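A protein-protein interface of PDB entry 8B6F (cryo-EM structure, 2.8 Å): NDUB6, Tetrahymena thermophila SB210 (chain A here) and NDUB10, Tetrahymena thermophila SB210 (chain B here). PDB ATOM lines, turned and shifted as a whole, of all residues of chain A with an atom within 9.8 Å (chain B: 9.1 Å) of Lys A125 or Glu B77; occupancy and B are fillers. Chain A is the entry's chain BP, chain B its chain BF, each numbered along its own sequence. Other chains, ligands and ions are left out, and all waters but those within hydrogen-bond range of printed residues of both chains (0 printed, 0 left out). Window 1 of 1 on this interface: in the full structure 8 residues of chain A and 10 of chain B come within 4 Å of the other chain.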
ATOM      1  N   VAL A 116     -13.913  30.957 -28.725  1.00  0.00           N
ATOM      2  CA  VAL A 116     -14.160  31.240 -27.316  1.00  0.00           C
ATOM      3  C   VAL A 116     -12.831  31.546 -26.643  1.00  0.00           C
ATOM      4  O   VAL A 116     -11.927  30.705 -26.620  1.00  0.00           O
ATOM      5  CB  VAL A 116     -14.869  30.063 -26.629  1.00  0.00           C
ATOM      6  CG1 VAL A 116     -15.046  30.331 -25.140  1.00  0.00           C
ATOM      7  CG2 VAL A 116     -16.212  29.800 -27.287  1.00  0.00           C
ATOM      8  N   ASP A 117     -12.712  32.746 -26.098  1.00  0.00           N
ATOM      9  CA  ASP A 117     -11.505  33.132 -25.381  1.00  0.00           C
ATOM     10  C   ASP A 117     -11.443  32.379 -24.057  1.00  0.00           C
ATOM     11  O   ASP A 117     -12.377  32.486 -23.253  1.00  0.00           O
ATOM     12  CB  ASP A 117     -11.499  34.637 -25.146  1.00  0.00           C
ATOM     13  CG  ASP A 117     -10.268  35.105 -24.404  1.00  0.00           C
ATOM     14  OD1 ASP A 117      -9.161  35.021 -24.972  1.00  0.00           O
ATOM     15  OD2 ASP A 117     -10.407  35.564 -23.254  1.00  0.00           O
ATOM     16  N   PRO A 118     -10.382  31.616 -23.782  1.00  0.00           N
ATOM     17  CA  PRO A 118     -10.375  30.808 -22.552  1.00  0.00           C
ATOM     18  C   PRO A 118     -10.477  31.628 -21.277  1.00  0.00           C
ATOM     19  O   PRO A 118     -10.979  31.118 -20.269  1.00  0.00           O
ATOM     20  CB  PRO A 118      -9.040  30.052 -22.638  1.00  0.00           C
ATOM     21  CG  PRO A 118      -8.196  30.861 -23.548  1.00  0.00           C
ATOM     22  CD  PRO A 118      -9.130  31.469 -24.544  1.00  0.00           C
ATOM     23  N   GLN A 119     -10.013  32.875 -21.284  1.00  0.00           N
ATOM     24  CA  GLN A 119     -10.043  33.718 -20.095  1.00  0.00           C
ATOM     25  C   GLN A 119     -11.295  34.581 -20.001  1.00  0.00           C
ATOM     26  O   GLN A 119     -11.458  35.298 -19.008  1.00  0.00           O
ATOM     27  CB  GLN A 119      -8.802  34.615 -20.052  1.00  0.00           C
ATOM     28  CG  GLN A 119      -7.563  33.926 -19.497  1.00  0.00           C
ATOM     29  CD  GLN A 119      -7.168  32.699 -20.290  1.00  0.00           C
ATOM     30  OE1 GLN A 119      -6.529  32.800 -21.336  1.00  0.00           O
ATOM     31  NE2 GLN A 119      -7.548  31.527 -19.794  1.00  0.00           N
ATOM     32  N   SER A 120     -12.176  34.539 -20.995  1.00  0.00           N
ATOM     33  CA  SER A 120     -13.405  35.306 -20.916  1.00  0.00           C
ATOM     34  C   SER A 120     -14.327  34.691 -19.864  1.00  0.00           C
ATOM     35  O   SER A 120     -14.255  33.490 -19.593  1.00  0.00           O
ATOM     36  CB  SER A 120     -14.107  35.345 -22.269  1.00  0.00           C
ATOM     37  OG  SER A 120     -14.402  34.040 -22.731  1.00  0.00           O
ATOM     38  N   PRO A 121     -15.204  35.492 -19.252  1.00  0.00           N
ATOM     39  CA  PRO A 121     -16.104  34.926 -18.235  1.00  0.00           C
ATOM     40  C   PRO A 121     -16.961  33.786 -18.753  1.00  0.00           C
ATOM     41  O   PRO A 121     -17.240  32.842 -18.005  1.00  0.00           O
ATOM     42  CB  PRO A 121     -16.959  36.131 -17.819  1.00  0.00           C
ATOM     43  CG  PRO A 121     -16.131  37.318 -18.152  1.00  0.00           C
ATOM     44  CD  PRO A 121     -15.366  36.950 -19.384  1.00  0.00           C
ATOM     45  N   VAL A 122     -17.388  33.843 -20.016  1.00  0.00           N
ATOM     46  CA  VAL A 122     -18.254  32.804 -20.564  1.00  0.00           C
ATOM     47  C   VAL A 122     -17.541  31.463 -20.612  1.00  0.00           C
ATOM     48  O   VAL A 122     -18.184  30.407 -20.567  1.00  0.00           O
ATOM     49  CB  VAL A 122     -18.759  33.224 -21.954  1.00  0.00           C
ATOM     50  CG1 VAL A 122     -19.610  32.129 -22.584  1.00  0.00           C
ATOM     51  CG2 VAL A 122     -19.544  34.495 -21.832  1.00  0.00           C
ATOM     52  N   ALA A 123     -16.217  31.472 -20.710  1.00  0.00           N
ATOM     53  CA  ALA A 123     -15.482  30.223 -20.767  1.00  0.00           C
ATOM     54  C   ALA A 123     -15.683  29.446 -19.468  1.00  0.00           C
ATOM     55  O   ALA A 123     -15.822  30.040 -18.394  1.00  0.00           O
ATOM     56  CB  ALA A 123     -13.996  30.486 -20.996  1.00  0.00           C
ATOM     57  N   PRO A 124     -15.702  28.116 -19.533  1.00  0.00           N
ATOM     58  CA  PRO A 124     -15.943  27.329 -18.318  1.00  0.00           C
ATOM     59  C   PRO A 124     -14.882  27.591 -17.262  1.00  0.00           C
ATOM     60  O   PRO A 124     -13.708  27.802 -17.568  1.00  0.00           O
ATOM     61  CB  PRO A 124     -15.900  25.879 -18.819  1.00  0.00           C
ATOM     62  CG  PRO A 124     -15.140  25.935 -20.087  1.00  0.00           C
ATOM     63  CD  PRO A 124     -15.453  27.259 -20.703  1.00  0.00           C
ATOM     64  N   LYS A 125     -15.316  27.580 -16.003  1.00  0.00           N
ATOM     65  CA  LYS A 125     -14.456  27.875 -14.867  1.00  0.00           C
ATOM     66  C   LYS A 125     -14.520  26.726 -13.874  1.00  0.00           C
ATOM     67  O   LYS A 125     -15.609  26.244 -13.547  1.00  0.00           O
ATOM     68  CB  LYS A 125     -14.872  29.184 -14.185  1.00  0.00           C
ATOM     69  CG  LYS A 125     -14.751  30.408 -15.077  1.00  0.00           C
ATOM     70  CD  LYS A 125     -15.051  31.686 -14.310  1.00  0.00           C
ATOM     71  CE  LYS A 125     -14.914  32.908 -15.205  1.00  0.00           C
ATOM     72  NZ  LYS A 125     -15.180  34.175 -14.469  1.00  0.00           N
ATOM     73  N   ALA A 126     -13.358  26.289 -13.403  1.00  0.00           N
ATOM     74  CA  ALA A 126     -13.291  25.214 -12.429  1.00  0.00           C
ATOM     75  C   ALA A 126     -13.621  25.735 -11.033  1.00  0.00           C
ATOM     76  O   ALA A 126     -13.519  26.930 -10.746  1.00  0.00           O
ATOM     77  CB  ALA A 126     -11.906  24.571 -12.436  1.00  0.00           C
ATOM     78  N   ILE A 127     -14.019  24.813 -10.156  1.00  0.00           N
ATOM     79  CA  ILE A 127     -14.359  25.175  -8.787  1.00  0.00           C
ATOM     80  C   ILE A 127     -13.093  25.560  -8.035  1.00  0.00           C
ATOM     81  O   ILE A 127     -12.054  24.898  -8.146  1.00  0.00           O
ATOM     82  CB  ILE A 127     -15.090  24.016  -8.087  1.00  0.00           C
ATOM     83  CG1 ILE A 127     -16.368  23.640  -8.843  1.00  0.00           C
ATOM     84  CG2 ILE A 127     -15.411  24.376  -6.642  1.00  0.00           C
ATOM     85  CD1 ILE A 127     -17.397  24.749  -8.932  1.00  0.00           C
ATOM     86  N   LYS A 128     -13.177  26.640  -7.261  1.00  0.00           N
ATOM     87  CA  LYS A 128     -12.061  27.129  -6.459  1.00  0.00           C
ATOM     88  C   LYS A 128     -12.325  26.764  -5.003  1.00  0.00           C
ATOM     89  O   LYS A 128     -13.240  27.306  -4.376  1.00  0.00           O
ATOM     90  CB  LYS A 128     -11.893  28.637  -6.627  1.00  0.00           C
ATOM     91  CG  LYS A 128     -10.729  29.222  -5.848  1.00  0.00           C
ATOM     92  CD  LYS A 128     -10.629  30.722  -6.070  1.00  0.00           C
ATOM     93  CE  LYS A 128      -9.449  31.315  -5.322  1.00  0.00           C
ATOM     94  NZ  LYS A 128      -9.339  32.784  -5.543  1.00  0.00           N
ATOM     95  N   GLU B  69     -23.400  20.469  -4.170  1.00  0.00           N
ATOM     96  CA  GLU B  69     -23.486  21.643  -5.033  1.00  0.00           C
ATOM     97  C   GLU B  69     -22.200  21.832  -5.825  1.00  0.00           C
ATOM     98  O   GLU B  69     -22.240  22.213  -6.999  1.00  0.00           O
ATOM     99  CB  GLU B  69     -23.793  22.886  -4.197  1.00  0.00           C
ATOM    100  CG  GLU B  69     -24.076  24.134  -5.020  1.00  0.00           C
ATOM    101  CD  GLU B  69     -25.331  24.009  -5.863  1.00  0.00           C
ATOM    102  OE1 GLU B  69     -26.130  23.085  -5.612  1.00  0.00           O
ATOM    103  OE2 GLU B  69     -25.519  24.837  -6.778  1.00  0.00           O
ATOM    104  N   TYR B  70     -21.047  21.578  -5.204  1.00  0.00           N
ATOM    105  CA  TYR B  70     -19.795  21.590  -5.953  1.00  0.00           C
ATOM    106  C   TYR B  70     -19.853  20.607  -7.115  1.00  0.00           C
ATOM    107  O   TYR B  70     -19.456  20.932  -8.238  1.00  0.00           O
ATOM    108  CB  TYR B  70     -18.622  21.245  -5.031  1.00  0.00           C
ATOM    109  CG  TYR B  70     -18.067  22.400  -4.226  1.00  0.00           C
ATOM    110  CD1 TYR B  70     -18.622  23.667  -4.308  1.00  0.00           C
ATOM    111  CD2 TYR B  70     -16.963  22.223  -3.404  1.00  0.00           C
ATOM    112  CE1 TYR B  70     -18.111  24.714  -3.586  1.00  0.00           C
ATOM    113  CE2 TYR B  70     -16.442  23.273  -2.673  1.00  0.00           C
ATOM    114  CZ  TYR B  70     -17.024  24.519  -2.775  1.00  0.00           C
ATOM    115  OH  TYR B  70     -16.547  25.597  -2.071  1.00  0.00           O
ATOM    116  N   ARG B  71     -20.339  19.391  -6.860  1.00  0.00           N
ATOM    117  CA  ARG B  71     -20.422  18.399  -7.924  1.00  0.00           C
ATOM    118  C   ARG B  71     -21.369  18.858  -9.027  1.00  0.00           C
ATOM    119  O   ARG B  71     -21.083  18.684 -10.216  1.00  0.00           O
ATOM    120  CB  ARG B  71     -20.871  17.055  -7.353  1.00  0.00           C
ATOM    121  CG  ARG B  71     -20.702  15.886  -8.311  1.00  0.00           C
ATOM    122  CD  ARG B  71     -19.236  15.679  -8.653  1.00  0.00           C
ATOM    123  NE  ARG B  71     -18.993  14.421  -9.349  1.00  0.00           N
ATOM    124  CZ  ARG B  71     -18.986  14.275 -10.666  1.00  0.00           C
ATOM    125  NH1 ARG B  71     -19.221  15.293 -11.477  1.00  0.00           N
ATOM    126  NH2 ARG B  71     -18.733  13.077 -11.183  1.00  0.00           N
ATOM    127  N   LYS B  72     -22.522  19.411  -8.649  1.00  0.00           N
ATOM    128  CA  LYS B  72     -23.466  19.899  -9.646  1.00  0.00           C
ATOM    129  C   LYS B  72     -22.866  21.034 -10.464  1.00  0.00           C
ATOM    130  O   LYS B  72     -23.058  21.102 -11.682  1.00  0.00           O
ATOM    131  CB  LYS B  72     -24.755  20.354  -8.964  1.00  0.00           C
ATOM    132  CG  LYS B  72     -25.510  19.233  -8.275  1.00  0.00           C
ATOM    133  CD  LYS B  72     -26.433  19.762  -7.190  1.00  0.00           C
ATOM    134  CE  LYS B  72     -27.469  20.719  -7.754  1.00  0.00           C
ATOM    135  NZ  LYS B  72     -28.384  21.219  -6.694  1.00  0.00           N
ATOM    136  N   ARG B  73     -22.139  21.940  -9.807  1.00  0.00           N
ATOM    137  CA  ARG B  73     -21.526  23.055 -10.520  1.00  0.00           C
ATOM    138  C   ARG B  73     -20.469  22.577 -11.507  1.00  0.00           C
ATOM    139  O   ARG B  73     -20.399  23.074 -12.637  1.00  0.00           O
ATOM    140  CB  ARG B  73     -20.913  24.036  -9.522  1.00  0.00           C
ATOM    141  CG  ARG B  73     -21.929  24.715  -8.623  1.00  0.00           C
ATOM    142  CD  ARG B  73     -22.638  25.853  -9.332  1.00  0.00           C
ATOM    143  NE  ARG B  73     -23.623  26.486  -8.463  1.00  0.00           N
ATOM    144  CZ  ARG B  73     -24.291  27.591  -8.762  1.00  0.00           C
ATOM    145  NH1 ARG B  73     -24.103  28.225  -9.907  1.00  0.00           N
ATOM    146  NH2 ARG B  73     -25.170  28.073  -7.888  1.00  0.00           N
ATOM    147  N   ILE B  74     -19.642  21.609 -11.111  1.00  0.00           N
ATOM    148  CA  ILE B  74     -18.611  21.120 -12.020  1.00  0.00           C
ATOM    149  C   ILE B  74     -19.243  20.372 -13.187  1.00  0.00           C
ATOM    150  O   ILE B  74     -18.764  20.455 -14.322  1.00  0.00           O
ATOM    151  CB  ILE B  74     -17.582  20.256 -11.262  1.00  0.00           C
ATOM    152  CG1 ILE B  74     -16.339  20.009 -12.119  1.00  0.00           C
ATOM    153  CG2 ILE B  74     -18.170  18.931 -10.837  1.00  0.00           C
ATOM    154  CD1 ILE B  74     -15.500  21.247 -12.341  1.00  0.00           C
ATOM    155  N   ASN B  75     -20.334  19.645 -12.936  1.00  0.00           N
ATOM    156  CA  ASN B  75     -21.052  18.998 -14.031  1.00  0.00           C
ATOM    157  C   ASN B  75     -21.618  20.028 -14.999  1.00  0.00           C
ATOM    158  O   ASN B  75     -21.550  19.847 -16.220  1.00  0.00           O
ATOM    159  CB  ASN B  75     -22.169  18.110 -13.483  1.00  0.00           C
ATOM    160  CG  ASN B  75     -21.649  16.837 -12.851  1.00  0.00           C
ATOM    161  OD1 ASN B  75     -20.726  16.209 -13.367  1.00  0.00           O
ATOM    162  ND2 ASN B  75     -22.244  16.443 -11.734  1.00  0.00           N
ATOM    163  N   ASN B  76     -22.187  21.113 -14.472  1.00  0.00           N
ATOM    164  CA  ASN B  76     -22.706  22.170 -15.333  1.00  0.00           C
ATOM    165  C   ASN B  76     -21.590  22.815 -16.141  1.00  0.00           C
ATOM    166  O   ASN B  76     -21.780  23.159 -17.314  1.00  0.00           O
ATOM    167  CB  ASN B  76     -23.438  23.220 -14.496  1.00  0.00           C
ATOM    168  CG  ASN B  76     -24.626  22.649 -13.755  1.00  0.00           C
ATOM    169  OD1 ASN B  76     -25.231  21.671 -14.192  1.00  0.00           O
ATOM    170  ND2 ASN B  76     -24.975  23.264 -12.632  1.00  0.00           N
ATOM    171  N   GLU B  77     -20.420  22.999 -15.529  1.00  0.00           N
ATOM    172  CA  GLU B  77     -19.281  23.551 -16.254  1.00  0.00           C
ATOM    173  C   GLU B  77     -18.826  22.610 -17.363  1.00  0.00           C
ATOM    174  O   GLU B  77     -18.410  23.062 -18.436  1.00  0.00           O
ATOM    175  CB  GLU B  77     -18.135  23.837 -15.285  1.00  0.00           C
ATOM    176  CG  GLU B  77     -18.427  24.964 -14.307  1.00  0.00           C
ATOM    177  CD  GLU B  77     -18.599  26.304 -14.993  1.00  0.00           C
ATOM    178  OE1 GLU B  77     -18.256  26.410 -16.187  1.00  0.00           O
ATOM    179  OE2 GLU B  77     -19.080  27.251 -14.338  1.00  0.00           O
ATOM    180  N   VAL B  78     -18.885  21.300 -17.123  1.00  0.00           N
ATOM    181  CA  VAL B  78     -18.540  20.343 -18.171  1.00  0.00           C
ATOM    182  C   VAL B  78     -19.526  20.443 -19.327  1.00  0.00           C
ATOM    183  O   VAL B  78     -19.139  20.379 -20.499  1.00  0.00           O
ATOM    184  CB  VAL B  78     -18.494  18.916 -17.597  1.00  0.00           C
ATOM    185  CG1 VAL B  78     -18.346  17.885 -18.707  1.00  0.00           C
ATOM    186  CG2 VAL B  78     -17.362  18.784 -16.626  1.00  0.00           C
ATOM    187  N   ARG B  79     -20.817  20.584 -19.018  1.00  0.00           N
ATOM    188  CA  ARG B  79     -21.801  20.779 -20.076  1.00  0.00           C
ATOM    189  C   ARG B  79     -21.518  22.058 -20.851  1.00  0.00           C
ATOM    190  O   ARG B  79     -21.613  22.083 -22.082  1.00  0.00           O
ATOM    191  CB  ARG B  79     -23.209  20.809 -19.483  1.00  0.00           C
ATOM    192  CG  ARG B  79     -24.293  21.173 -20.485  1.00  0.00           C
ATOM    193  CD  ARG B  79     -25.662  21.156 -19.835  1.00  0.00           C
ATOM    194  NE  ARG B  79     -25.763  22.121 -18.748  1.00  0.00           N
ATOM    195  CZ  ARG B  79     -26.742  22.142 -17.854  1.00  0.00           C
ATOM    196  NH1 ARG B  79     -27.723  21.254 -17.880  1.00  0.00           N
ATOM    197  NH2 ARG B  79     -26.737  23.077 -16.908  1.00  0.00           N
ATOM    198  N   ARG B  80     -21.180  23.136 -20.140  1.00  0.00           N
ATOM    199  CA  ARG B  80     -20.850  24.391 -20.807  1.00  0.00           C
ATOM    200  C   ARG B  80     -19.642  24.221 -21.716  1.00  0.00           C
ATOM    201  O   ARG B  80     -19.632  24.714 -22.850  1.00  0.00           O
ATOM    202  CB  ARG B  80     -20.594  25.478 -19.763  1.00  0.00           C
ATOM    203  CG  ARG B  80     -20.046  26.783 -20.320  1.00  0.00           C
ATOM    204  CD  ARG B  80     -19.660  27.725 -19.198  1.00  0.00           C
ATOM    205  NE  ARG B  80     -20.827  28.189 -18.456  1.00  0.00           N
ATOM    206  CZ  ARG B  80     -21.498  29.301 -18.720  1.00  0.00           C
ATOM    207  NH1 ARG B  80     -21.144  30.108 -19.705  1.00  0.00           N
ATOM    208  NH2 ARG B  80     -22.549  29.616 -17.969  1.00  0.00           N
ATOM    209  N   ALA B  81     -18.614  23.522 -21.237  1.00  0.00           N
ATOM    210  CA  ALA B  81     -17.442  23.264 -22.063  1.00  0.00           C
ATOM    211  C   ALA B  81     -17.807  22.452 -23.295  1.00  0.00           C
ATOM    212  O   ALA B  81     -17.328  22.735 -24.399  1.00  0.00           O
ATOM    213  CB  ALA B  81     -16.375  22.539 -21.244  1.00  0.00           C
ATOM    214  N   ALA B  82     -18.652  21.434 -23.129  1.00  0.00           N
ATOM    215  CA  ALA B  82     -19.048  20.616 -24.269  1.00  0.00           C
ATOM    216  C   ALA B  82     -19.769  21.442 -25.327  1.00  0.00           C
ATOM    217  O   ALA B  82     -19.526  21.273 -26.527  1.00  0.00           O
ATOM    218  CB  ALA B  82     -19.935  19.466 -23.794  1.00  0.00           C
ATOM    219  N   ILE B  83     -20.669  22.329 -24.905  1.00  0.00           N
ATOM    220  CA  ILE B  83     -21.422  23.125 -25.871  1.00  0.00           C
ATOM    221  C   ILE B  83     -20.520  24.155 -26.543  1.00  0.00           C
ATOM    222  O   ILE B  83     -20.577  24.342 -27.762  1.00  0.00           O
ATOM    223  CB  ILE B  83     -22.648  23.769 -25.194  1.00  0.00           C
ATOM    224  CG1 ILE B  83     -23.627  22.665 -24.774  1.00  0.00           C
ATOM    225  CG2 ILE B  83     -23.319  24.777 -26.126  1.00  0.00           C
ATOM    226  CD1 ILE B  83     -24.861  23.142 -24.058  1.00  0.00           C
ATOM    227  N   LEU B  84     -19.682  24.843 -25.765  1.00  0.00           N
ATOM    228  CA  LEU B  84     -18.887  25.931 -26.328  1.00  0.00           C
ATOM    229  C   LEU B  84     -17.760  25.400 -27.207  1.00  0.00           C
ATOM    230  O   LEU B  84     -17.546  25.892 -28.321  1.00  0.00           O
ATOM    231  CB  LEU B  84     -18.321  26.801 -25.204  1.00  0.00           C
ATOM    232  CG  LEU B  84     -19.335  27.597 -24.378  1.00  0.00           C
ATOM    233  CD1 LEU B  84     -18.641  28.304 -23.229  1.00  0.00           C
ATOM    234  CD2 LEU B  84     -20.087  28.596 -25.241  1.00  0.00           C
ATOM    235  N   THR B  85     -17.027  24.395 -26.727  1.00  0.00           N
ATOM    236  CA  THR B  85     -15.820  23.940 -27.412  1.00  0.00           C
ATOM    237  C   THR B  85     -16.143  22.769 -28.334  1.00  0.00           C
ATOM    238  O   THR B  85     -16.837  21.836 -27.915  1.00  0.00           O
ATOM    239  CB  THR B  85     -14.754  23.519 -26.410  1.00  0.00           C
ATOM    240  OG1 THR B  85     -14.485  24.596 -25.506  1.00  0.00           O
ATOM    241  CG2 THR B  85     -13.464  23.133 -27.120  1.00  0.00           C
ATOM    242  N   LEU B  90     -11.487  19.416 -27.142  1.00  0.00           N
ATOM    243  CA  LEU B  90     -12.332  19.404 -25.953  1.00  0.00           C
ATOM    244  C   LEU B  90     -11.695  18.584 -24.837  1.00  0.00           C
ATOM    245  O   LEU B  90     -11.604  19.040 -23.692  1.00  0.00           O
ATOM    246  CB  LEU B  90     -13.719  18.862 -26.298  1.00  0.00           C
ATOM    247  CG  LEU B  90     -14.686  18.693 -25.121  1.00  0.00           C
ATOM    248  CD1 LEU B  90     -14.791  19.967 -24.301  1.00  0.00           C
ATOM    249  CD2 LEU B  90     -16.056  18.276 -25.622  1.00  0.00           C
ATOM    250  N   MET B  94     -10.103  19.660 -21.306  1.00  0.00           N
ATOM    251  CA  MET B  94     -10.656  19.054 -20.101  1.00  0.00           C
ATOM    252  C   MET B  94      -9.590  18.372 -19.260  1.00  0.00           C
ATOM    253  O   MET B  94      -9.737  18.289 -18.037  1.00  0.00           O
ATOM    254  CB  MET B  94     -11.747  18.045 -20.459  1.00  0.00           C
ATOM    255  CG  MET B  94     -13.077  18.679 -20.823  1.00  0.00           C
ATOM    256  SD  MET B  94     -14.399  17.470 -21.027  1.00  0.00           S
ATOM    257  CE  MET B  94     -14.508  16.785 -19.374  1.00  0.00           C
ATOM    258  N   LYS B  97      -7.425  21.302 -14.703  1.00  0.00           N
ATOM    259  CA  LYS B  97      -8.087  21.443 -13.410  1.00  0.00           C
ATOM    260  C   LYS B  97      -9.452  20.764 -13.392  1.00  0.00           C
ATOM    261  O   LYS B  97      -9.829  20.148 -12.390  1.00  0.00           O
ATOM    262  CB  LYS B  97      -8.243  22.922 -13.049  1.00  0.00           C
ATOM    263  CG  LYS B  97      -6.931  23.672 -12.914  1.00  0.00           C
ATOM    264  CD  LYS B  97      -7.166  25.128 -12.546  1.00  0.00           C
ATOM    265  CE  LYS B  97      -5.849  25.863 -12.352  1.00  0.00           C
ATOM    266  NZ  LYS B  97      -6.056  27.295 -11.991  1.00  0.00           N
ATOM    267  N   ILE B  98     -10.197  20.865 -14.492  1.00  0.00           N
ATOM    268  CA  ILE B  98     -11.594  20.437 -14.492  1.00  0.00           C
ATOM    269  C   ILE B  98     -11.701  18.927 -14.297  1.00  0.00           C
ATOM    270  O   ILE B  98     -12.492  18.449 -13.477  1.00  0.00           O
ATOM    271  CB  ILE B  98     -12.297  20.907 -15.781  1.00  0.00           C
ATOM    272  CG1 ILE B  98     -13.791  20.578 -15.718  1.00  0.00           C
ATOM    273  CG2 ILE B  98     -11.663  20.277 -17.010  1.00  0.00           C
ATOM    274  CD1 ILE B  98     -14.593  21.123 -16.881  1.00  0.00           C
ATOM    275  N   GLN B 101     -10.784  17.906 -10.736  1.00  0.00           N
ATOM    276  CA  GLN B 101     -11.861  18.230  -9.806  1.00  0.00           C
ATOM    277  C   GLN B 101     -13.031  17.267  -9.949  1.00  0.00           C
ATOM    278  O   GLN B 101     -13.640  16.875  -8.948  1.00  0.00           O
ATOM    279  CB  GLN B 101     -12.322  19.672 -10.018  1.00  0.00           C
ATOM    280  CG  GLN B 101     -11.310  20.710  -9.554  1.00  0.00           C
ATOM    281  CD  GLN B 101     -11.838  22.123  -9.659  1.00  0.00           C
ATOM    282  OE1 GLN B 101     -12.969  22.346 -10.085  1.00  0.00           O
ATOM    283  NE2 GLN B 101     -11.018  23.091  -9.262  1.00  0.00           N
ATOM    284  N   ILE B 102     -13.364  16.874 -11.178  1.00  0.00           N
ATOM    285  CA  ILE B 102     -14.447  15.914 -11.377  1.00  0.00           C
ATOM    286  C   ILE B 102     -14.144  14.620 -10.633  1.00  0.00           C
ATOM    287  O   ILE B 102     -15.001  14.065  -9.937  1.00  0.00           O
ATOM    288  CB  ILE B 102     -14.646  15.655 -12.880  1.00  0.00           C
ATOM    289  CG1 ILE B 102     -15.205  16.903 -13.555  1.00  0.00           C
ATOM    290  CG2 ILE B 102     -15.581  14.472 -13.110  1.00  0.00           C
ATOM    291  CD1 ILE B 102     -15.108  16.855 -15.053  1.00  0.00           C
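Of the 23 printed residues of chain B, 6 touch a printed residue of chain A. Printed residues of chain B that touch a printed residue of chain A: Arg B73, Glu B77, Arg B80, Ala B81, Leu B84 and Gln B101. Among the printed residues, 9 pairs touch across the chains. Among the printed residues, no Asp or Glu carboxylate lies within 4 Å of a Lys or Arg side-chain nitrogen of the other chain.
Val A122 touches Leu B84. Glu B77 touches Pro A124. CA of Pro A124 touches CD of Arg B80, at 3.8 Å. CG of Pro A124 touches CB of Ala B81, at 3.8 Å. Gln B101 touches Ala A126. CD1 of Ile A127 touches CB of Arg B73, at 3.6 Å.
N of Ile A127 is in hydrogen-bond range of OE1 of Gln B101, 2.7 Å away. The backbone carbonyl oxygen (O) of Val A122 lies within hydrogen-bond range of the guanidinium group (NH1) of Arg B80 (3.1 Å). OE1 of Glu B77 is in hydrogen-bond range of N of Lys A125.
The side-chain carboxylate of Glu B69 is in salt-bridge range of the guanidinium group of Arg B73 (3.0 Å). The side-chain carboxylate (OE1) of Glu B77 is in salt-bridge range of the guanidinium group (NE) of Arg B80.
Of chain B, only Glu B77 comes within 4 Å of Lys A125. Glu B77 touches two residues of chain A. Pro A124 touches just these residues of chain B: Glu B77 (3.3 Å), Arg B80 (3.8 Å) and Ala B81 (3.8 Å). Ala A126 touches just one residue of chain B: Gln B101. No residue of chain A comes within 4 Å of Val B78. Of the printed residues of chain B, Ile A127 touches Arg B73 and Gln B101. Of the printed residues of chain A, Arg B73 touches Ile A127 (3.6 Å). Printed residues of chain A within 4 Å of Leu B84: Val A122 (3.4 Å). Gln A119 touches none of the printed residues of chain B. The nearest residue of chain A that does not touch Glu B77 is Ala A123 (4.9 Å).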
